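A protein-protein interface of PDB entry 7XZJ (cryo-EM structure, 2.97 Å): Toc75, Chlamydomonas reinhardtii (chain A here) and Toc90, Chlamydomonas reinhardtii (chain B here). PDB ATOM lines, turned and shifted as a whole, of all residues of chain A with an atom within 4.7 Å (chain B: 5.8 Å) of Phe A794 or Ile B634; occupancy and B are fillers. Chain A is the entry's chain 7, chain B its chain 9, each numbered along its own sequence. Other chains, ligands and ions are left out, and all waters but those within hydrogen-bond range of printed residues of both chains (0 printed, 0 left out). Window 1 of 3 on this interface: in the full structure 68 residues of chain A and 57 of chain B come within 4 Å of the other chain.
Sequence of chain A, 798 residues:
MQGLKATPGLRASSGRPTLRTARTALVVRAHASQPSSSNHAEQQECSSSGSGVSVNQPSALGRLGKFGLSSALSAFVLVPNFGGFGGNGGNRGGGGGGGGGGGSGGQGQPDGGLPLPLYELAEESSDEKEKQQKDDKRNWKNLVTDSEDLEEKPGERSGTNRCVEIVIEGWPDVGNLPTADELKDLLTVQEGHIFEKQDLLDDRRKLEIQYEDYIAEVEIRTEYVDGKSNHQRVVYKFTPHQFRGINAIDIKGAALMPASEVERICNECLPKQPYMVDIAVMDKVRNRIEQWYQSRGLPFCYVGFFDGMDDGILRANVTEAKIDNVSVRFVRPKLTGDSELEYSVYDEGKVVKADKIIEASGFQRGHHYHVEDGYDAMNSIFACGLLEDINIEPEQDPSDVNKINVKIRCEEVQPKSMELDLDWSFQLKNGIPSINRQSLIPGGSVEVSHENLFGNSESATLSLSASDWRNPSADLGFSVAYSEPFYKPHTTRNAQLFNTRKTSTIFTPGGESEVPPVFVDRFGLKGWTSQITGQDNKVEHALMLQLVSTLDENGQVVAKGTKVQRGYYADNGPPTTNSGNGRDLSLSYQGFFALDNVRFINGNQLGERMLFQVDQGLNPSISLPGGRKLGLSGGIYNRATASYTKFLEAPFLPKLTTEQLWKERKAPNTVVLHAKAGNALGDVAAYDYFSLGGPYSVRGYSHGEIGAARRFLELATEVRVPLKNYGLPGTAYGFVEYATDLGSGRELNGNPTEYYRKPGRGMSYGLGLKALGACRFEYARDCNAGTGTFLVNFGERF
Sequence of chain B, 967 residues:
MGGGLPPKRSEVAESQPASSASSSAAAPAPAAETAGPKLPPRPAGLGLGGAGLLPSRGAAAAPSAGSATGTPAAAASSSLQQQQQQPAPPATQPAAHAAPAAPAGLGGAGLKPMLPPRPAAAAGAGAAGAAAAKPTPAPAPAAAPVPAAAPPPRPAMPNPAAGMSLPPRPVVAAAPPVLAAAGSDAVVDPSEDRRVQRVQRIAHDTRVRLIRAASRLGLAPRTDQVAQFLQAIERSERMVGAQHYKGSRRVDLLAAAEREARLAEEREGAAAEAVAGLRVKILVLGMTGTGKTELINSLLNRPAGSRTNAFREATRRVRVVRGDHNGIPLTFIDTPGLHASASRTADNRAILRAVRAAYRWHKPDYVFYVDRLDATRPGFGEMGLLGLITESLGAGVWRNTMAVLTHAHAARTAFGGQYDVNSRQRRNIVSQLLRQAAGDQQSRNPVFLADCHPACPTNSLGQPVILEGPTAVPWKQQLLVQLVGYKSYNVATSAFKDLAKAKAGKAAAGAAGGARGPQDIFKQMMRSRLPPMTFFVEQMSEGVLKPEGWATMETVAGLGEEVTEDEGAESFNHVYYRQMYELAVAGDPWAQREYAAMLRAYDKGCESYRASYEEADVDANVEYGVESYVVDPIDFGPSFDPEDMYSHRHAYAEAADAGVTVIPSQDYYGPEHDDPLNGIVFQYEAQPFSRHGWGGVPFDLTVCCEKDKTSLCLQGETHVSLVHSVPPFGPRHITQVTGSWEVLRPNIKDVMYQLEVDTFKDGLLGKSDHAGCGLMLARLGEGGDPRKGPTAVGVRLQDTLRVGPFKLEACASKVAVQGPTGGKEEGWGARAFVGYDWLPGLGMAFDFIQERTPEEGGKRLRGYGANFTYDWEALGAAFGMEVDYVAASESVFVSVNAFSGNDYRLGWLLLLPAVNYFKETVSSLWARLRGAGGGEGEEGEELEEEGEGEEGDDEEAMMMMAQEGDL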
ATOM      1  N   TYR A 696     -19.491  23.632  -5.034  1.00  0.00           N
ATOM      2  CA  TYR A 696     -19.779  24.639  -6.090  1.00  0.00           C
ATOM      3  C   TYR A 696     -19.100  25.948  -5.678  1.00  0.00           C
ATOM      4  O   TYR A 696     -18.545  25.973  -4.562  1.00  0.00           O
ATOM      5  CB  TYR A 696     -21.277  24.692  -6.395  1.00  0.00           C
ATOM      6  CG  TYR A 696     -21.769  23.451  -7.096  1.00  0.00           C
ATOM      7  CD1 TYR A 696     -21.639  23.309  -8.467  1.00  0.00           C
ATOM      8  CD2 TYR A 696     -22.323  22.399  -6.386  1.00  0.00           C
ATOM      9  CE1 TYR A 696     -22.069  22.167  -9.120  1.00  0.00           C
ATOM     10  CE2 TYR A 696     -22.758  21.247  -7.023  1.00  0.00           C
ATOM     11  CZ  TYR A 696     -22.631  21.131  -8.395  1.00  0.00           C
ATOM     12  OH  TYR A 696     -23.058  20.001  -9.030  1.00  0.00           O
ATOM     13  N   ALA A 774     -22.603  12.371 -15.201  1.00  0.00           N
ATOM     14  CA  ALA A 774     -22.092  13.675 -14.719  1.00  0.00           C
ATOM     15  C   ALA A 774     -21.051  13.457 -13.618  1.00  0.00           C
ATOM     16  O   ALA A 774     -20.580  14.457 -13.047  1.00  0.00           O
ATOM     17  CB  ALA A 774     -23.239  14.514 -14.227  1.00  0.00           C
ATOM     18  N   CYS A 775     -20.706  12.200 -13.338  1.00  0.00           N
ATOM     19  CA  CYS A 775     -19.745  11.907 -12.245  1.00  0.00           C
ATOM     20  C   CYS A 775     -18.391  12.531 -12.597  1.00  0.00           C
ATOM     21  O   CYS A 775     -17.987  12.436 -13.770  1.00  0.00           O
ATOM     22  CB  CYS A 775     -19.577  10.405 -12.077  1.00  0.00           C
ATOM     23  SG  CYS A 775     -21.156   9.519 -12.049  1.00  0.00           S
ATOM     24  N   ARG A 776     -17.725  13.139 -11.612  1.00  0.00           N
ATOM     25  CA  ARG A 776     -16.412  13.788 -11.864  1.00  0.00           C
ATOM     26  C   ARG A 776     -15.502  13.606 -10.646  1.00  0.00           C
ATOM     27  O   ARG A 776     -16.013  13.666  -9.512  1.00  0.00           O
ATOM     28  CB  ARG A 776     -16.591  15.257 -12.266  1.00  0.00           C
ATOM     29  CG  ARG A 776     -17.176  16.156 -11.187  1.00  0.00           C
ATOM     30  CD  ARG A 776     -17.554  17.516 -11.744  1.00  0.00           C
ATOM     31  NE  ARG A 776     -17.519  18.586 -10.757  1.00  0.00           N
ATOM     32  CZ  ARG A 776     -18.547  18.965 -10.007  1.00  0.00           C
ATOM     33  NH1 ARG A 776     -19.714  18.355 -10.120  1.00  0.00           N
ATOM     34  NH2 ARG A 776     -18.404  19.954  -9.143  1.00  0.00           N
ATOM     35  N   ASN A 793     -17.490  13.968  -7.028  1.00  0.00           N
ATOM     36  CA  ASN A 793     -18.777  14.715  -7.013  1.00  0.00           C
ATOM     37  C   ASN A 793     -19.639  14.306  -8.211  1.00  0.00           C
ATOM     38  O   ASN A 793     -19.066  13.930  -9.248  1.00  0.00           O
ATOM     39  CB  ASN A 793     -18.552  16.229  -6.995  1.00  0.00           C
ATOM     40  CG  ASN A 793     -19.737  16.994  -6.447  1.00  0.00           C
ATOM     41  OD1 ASN A 793     -20.659  16.404  -5.888  1.00  0.00           O
ATOM     42  ND2 ASN A 793     -19.721  18.309  -6.594  1.00  0.00           N
ATOM     43  N   PHE A 794     -20.963  14.383  -8.066  1.00  0.00           N
ATOM     44  CA  PHE A 794     -21.868  14.080  -9.202  1.00  0.00           C
ATOM     45  C   PHE A 794     -22.520  15.385  -9.655  1.00  0.00           C
ATOM     46  O   PHE A 794     -23.104  16.084  -8.808  1.00  0.00           O
ATOM     47  CB  PHE A 794     -22.937  13.069  -8.782  1.00  0.00           C
ATOM     48  CG  PHE A 794     -23.968  12.765  -9.838  1.00  0.00           C
ATOM     49  CD1 PHE A 794     -23.668  11.937 -10.907  1.00  0.00           C
ATOM     50  CD2 PHE A 794     -25.242  13.305  -9.766  1.00  0.00           C
ATOM     51  CE1 PHE A 794     -24.615  11.657 -11.879  1.00  0.00           C
ATOM     52  CE2 PHE A 794     -26.188  13.028 -10.740  1.00  0.00           C
ATOM     53  CZ  PHE A 794     -25.874  12.202 -11.793  1.00  0.00           C
ATOM     54  N   GLY A 795     -22.422  15.703 -10.948  1.00  0.00           N
ATOM     55  CA  GLY A 795     -23.074  16.916 -11.473  1.00  0.00           C
ATOM     56  C   GLY A 795     -22.154  17.735 -12.358  1.00  0.00           C
ATOM     57  O   GLY A 795     -20.973  17.363 -12.485  1.00  0.00           O
ATOM     58  N   ASP B 632     -32.830  13.973 -18.899  1.00  0.00           N
ATOM     59  CA  ASP B 632     -33.677  14.787 -18.040  1.00  0.00           C
ATOM     60  C   ASP B 632     -33.019  15.030 -16.683  1.00  0.00           C
ATOM     61  O   ASP B 632     -32.224  14.211 -16.212  1.00  0.00           O
ATOM     62  CB  ASP B 632     -35.025  14.109 -17.833  1.00  0.00           C
ATOM     63  CG  ASP B 632     -36.117  14.715 -18.685  1.00  0.00           C
ATOM     64  OD1 ASP B 632     -35.799  15.536 -19.568  1.00  0.00           O
ATOM     65  OD2 ASP B 632     -37.297  14.376 -18.464  1.00  0.00           O
ATOM     66  N   PRO B 633     -33.340  16.155 -16.031  1.00  0.00           N
ATOM     67  CA  PRO B 633     -32.797  16.419 -14.690  1.00  0.00           C
ATOM     68  C   PRO B 633     -33.415  15.540 -13.610  1.00  0.00           C
ATOM     69  O   PRO B 633     -34.216  14.647 -13.903  1.00  0.00           O
ATOM     70  CB  PRO B 633     -33.135  17.900 -14.459  1.00  0.00           C
ATOM     71  CG  PRO B 633     -33.463  18.451 -15.810  1.00  0.00           C
ATOM     72  CD  PRO B 633     -34.071  17.317 -16.563  1.00  0.00           C
ATOM     73  N   ILE B 634     -33.043  15.789 -12.356  1.00  0.00           N
ATOM     74  CA  ILE B 634     -33.504  15.010 -11.213  1.00  0.00           C
ATOM     75  C   ILE B 634     -34.455  15.867 -10.392  1.00  0.00           C
ATOM     76  O   ILE B 634     -34.117  16.995 -10.014  1.00  0.00           O
ATOM     77  CB  ILE B 634     -32.327  14.527 -10.350  1.00  0.00           C
ATOM     78  CG1 ILE B 634     -31.222  13.962 -11.239  1.00  0.00           C
ATOM     79  CG2 ILE B 634     -32.797  13.483  -9.352  1.00  0.00           C
ATOM     80  CD1 ILE B 634     -29.967  13.606 -10.487  1.00  0.00           C
ATOM     81  N   ASP B 635     -35.639  15.335 -10.115  1.00  0.00           N
ATOM     82  CA  ASP B 635     -36.624  16.053  -9.321  1.00  0.00           C
ATOM     83  C   ASP B 635     -36.289  15.965  -7.837  1.00  0.00           C
ATOM     84  O   ASP B 635     -35.868  14.917  -7.341  1.00  0.00           O
ATOM     85  CB  ASP B 635     -38.021  15.493  -9.576  1.00  0.00           C
ATOM     86  CG  ASP B 635     -39.109  16.331  -8.939  1.00  0.00           C
ATOM     87  OD1 ASP B 635     -38.839  17.501  -8.599  1.00  0.00           O
ATOM     88  OD2 ASP B 635     -40.234  15.818  -8.778  1.00  0.00           O
ATOM     89  N   PHE B 636     -36.486  17.078  -7.124  1.00  0.00           N
ATOM     90  CA  PHE B 636     -36.188  17.147  -5.700  1.00  0.00           C
ATOM     91  C   PHE B 636     -37.353  17.615  -4.840  1.00  0.00           C
ATOM     92  O   PHE B 636     -37.187  17.744  -3.622  1.00  0.00           O
ATOM     93  CB  PHE B 636     -34.987  18.070  -5.452  1.00  0.00           C
ATOM     94  CG  PHE B 636     -33.690  17.523  -5.962  1.00  0.00           C
ATOM     95  CD1 PHE B 636     -33.202  16.316  -5.492  1.00  0.00           C
ATOM     96  CD2 PHE B 636     -32.954  18.217  -6.903  1.00  0.00           C
ATOM     97  CE1 PHE B 636     -32.009  15.810  -5.958  1.00  0.00           C
ATOM     98  CE2 PHE B 636     -31.759  17.716  -7.372  1.00  0.00           C
ATOM     99  CZ  PHE B 636     -31.286  16.510  -6.899  1.00  0.00           C
ATOM    100  N   HIS B 650     -27.809  19.113 -13.555  1.00  0.00           N
ATOM    101  CA  HIS B 650     -28.325  17.750 -13.541  1.00  0.00           C
ATOM    102  C   HIS B 650     -28.713  17.241 -14.923  1.00  0.00           C
ATOM    103  O   HIS B 650     -29.208  16.116 -15.036  1.00  0.00           O
ATOM    104  CB  HIS B 650     -29.532  17.654 -12.606  1.00  0.00           C
ATOM    105  CG  HIS B 650     -29.261  18.150 -11.223  1.00  0.00           C
ATOM    106  ND1 HIS B 650     -28.426  17.492 -10.346  1.00  0.00           N
ATOM    107  CD2 HIS B 650     -29.710  19.244 -10.565  1.00  0.00           C
ATOM    108  CE1 HIS B 650     -28.376  18.157  -9.206  1.00  0.00           C
ATOM    109  NE2 HIS B 650     -29.147  19.224  -9.313  1.00  0.00           N
ATOM    110  N   TYR B 652     -27.193  16.305 -18.641  1.00  0.00           N
ATOM    111  CA  TYR B 652     -25.906  15.997 -19.245  1.00  0.00           C
ATOM    112  C   TYR B 652     -26.119  15.102 -20.457  1.00  0.00           C
ATOM    113  O   TYR B 652     -27.173  14.483 -20.621  1.00  0.00           O
ATOM    114  CB  TYR B 652     -24.966  15.325 -18.234  1.00  0.00           C
ATOM    115  CG  TYR B 652     -25.626  14.221 -17.440  1.00  0.00           C
ATOM    116  CD1 TYR B 652     -25.617  12.910 -17.896  1.00  0.00           C
ATOM    117  CD2 TYR B 652     -26.263  14.490 -16.235  1.00  0.00           C
ATOM    118  CE1 TYR B 652     -26.222  11.899 -17.176  1.00  0.00           C
ATOM    119  CE2 TYR B 652     -26.871  13.484 -15.509  1.00  0.00           C
ATOM    120  CZ  TYR B 652     -26.847  12.192 -15.983  1.00  0.00           C
ATOM    121  OH  TYR B 652     -27.451  11.188 -15.262  1.00  0.00           O
ATOM    122  N   VAL B 662     -24.831   4.471 -12.797  1.00  0.00           N
ATOM    123  CA  VAL B 662     -24.504   5.444 -11.714  1.00  0.00           C
ATOM    124  C   VAL B 662     -25.793   6.034 -11.136  1.00  0.00           C
ATOM    125  O   VAL B 662     -26.633   6.510 -11.919  1.00  0.00           O
ATOM    126  CB  VAL B 662     -23.527   6.528 -12.206  1.00  0.00           C
ATOM    127  CG1 VAL B 662     -22.126   5.965 -12.379  1.00  0.00           C
ATOM    128  CG2 VAL B 662     -23.995   7.180 -13.498  1.00  0.00           C
ATOM    129  N   PRO B 664     -27.195   8.832  -8.139  1.00  0.00           N
ATOM    130  CA  PRO B 664     -26.810   9.835  -7.142  1.00  0.00           C
ATOM    131  C   PRO B 664     -27.290   9.509  -5.718  1.00  0.00           C
ATOM    132  O   PRO B 664     -28.357   8.941  -5.579  1.00  0.00           O
ATOM    133  CB  PRO B 664     -27.484  11.115  -7.653  1.00  0.00           C
ATOM    134  CG  PRO B 664     -28.652  10.621  -8.475  1.00  0.00           C
ATOM    135  CD  PRO B 664     -28.153   9.347  -9.119  1.00  0.00           C
ATOM    136  N   ASP B 675     -27.475  22.014  -3.806  1.00  0.00           N
ATOM    137  CA  ASP B 675     -28.121  20.698  -4.063  1.00  0.00           C
ATOM    138  C   ASP B 675     -27.690  19.679  -2.985  1.00  0.00           C
ATOM    139  O   ASP B 675     -26.527  19.772  -2.547  1.00  0.00           O
ATOM    140  CB  ASP B 675     -27.865  20.212  -5.494  1.00  0.00           C
ATOM    141  CG  ASP B 675     -26.398  20.125  -5.889  1.00  0.00           C
ATOM    142  OD1 ASP B 675     -25.561  20.744  -5.205  1.00  0.00           O
ATOM    143  OD2 ASP B 675     -26.106  19.436  -6.886  1.00  0.00           O
ATOM    144  N   LEU B 677     -26.943  16.531  -3.203  1.00  0.00           N
ATOM    145  CA  LEU B 677     -26.381  15.299  -3.821  1.00  0.00           C
ATOM    146  C   LEU B 677     -24.901  15.163  -3.462  1.00  0.00           C
ATOM    147  O   LEU B 677     -24.092  15.940  -4.003  1.00  0.00           O
ATOM    148  CB  LEU B 677     -26.561  15.370  -5.339  1.00  0.00           C
ATOM    149  CG  LEU B 677     -27.988  15.176  -5.846  1.00  0.00           C
ATOM    150  CD1 LEU B 677     -27.999  15.053  -7.361  1.00  0.00           C
ATOM    151  CD2 LEU B 677     -28.621  13.948  -5.212  1.00  0.00           C
ATOM    152  N   GLY B 679     -21.737  12.349  -3.470  1.00  0.00           N
ATOM    153  CA  GLY B 679     -21.267  10.990  -3.801  1.00  0.00           C
ATOM    154  C   GLY B 679     -22.120  10.304  -4.854  1.00  0.00           C
ATOM    155  O   GLY B 679     -23.145  10.884  -5.263  1.00  0.00           O
ATOM    156  N   ILE B 680     -21.721   9.095  -5.264  1.00  0.00           N
ATOM    157  CA  ILE B 680     -22.478   8.332  -6.300  1.00  0.00           C
ATOM    158  C   ILE B 680     -22.507   6.855  -5.903  1.00  0.00           C
ATOM    159  O   ILE B 680     -21.611   6.436  -5.150  1.00  0.00           O
ATOM    160  CB  ILE B 680     -21.845   8.507  -7.696  1.00  0.00           C
ATOM    161  CG1 ILE B 680     -20.646   9.459  -7.688  1.00  0.00           C
ATOM    162  CG2 ILE B 680     -22.897   8.923  -8.712  1.00  0.00           C
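O of Ala A774 is in hydrogen-bond range of N of Gly A795. The backbone NH (N) of Arg A776 sits at hydrogen-bond distance from the backbone carbonyl oxygen (O) of Asn A793, at 2.8 Å.
Among the printed residues, merely in contact across the chains: Tyr A696 with Asp B675 (3.4 Å), Ala A774 with Tyr B652 (3.6 Å), Cys A775 with Val B662 (3.7 Å), Cys A775 with Ile B680 (3.8 Å), Asn A793 with Leu B677 (3.9 Å), Phe A794 with Ile B634 (3.8 Å), Phe A794 with Tyr B652 (3.9 Å), Phe A794 with Pro B664 (3.8 Å) and Phe A794 with Ile B680 (3.8 Å).
Of the printed residues of chain B, Tyr A696 touches Asp B675 (3.4 Å). Arg A776 touches none of the printed residues of chain B. Of chain B, only Ile B634, Tyr B652, Pro B664 and Ile B680 come within 4 Å of Phe A794. Of the printed residues of chain A, Ile B634 touches Phe A794. Of the printed residues of chain A, Val B662 touches Cys A775. Printed residues of chain A within 4 Å of Pro B664: Phe A794 (3.8 Å). The nearest residue of chain B that does not touch Phe A794 is Leu B677 (4.1 Å). The nearest printed residue of chain A that does not touch Ile B634 is Gly A795 (7.7 Å). The nearest printed residue of chain A that does not touch Pro B664 is Cys A775 (7.2 Å).
Hydrophobic or aromatic side chains of chain B that line the printed part of chain A: Ile B634, Tyr B652, Val B662, Pro B664 and Ile B680. Of the 7 printed residues of chain A, 5 touch a printed residue of chain B. Hydrophobic or aromatic side chains of chain A that line the printed part of chain B: Tyr A696, Ala A774 and Phe A794. Among the printed residues, no Asp or Glu carboxylate lies within 4 Å of a Lys or Arg side-chain nitrogen of the other chain.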
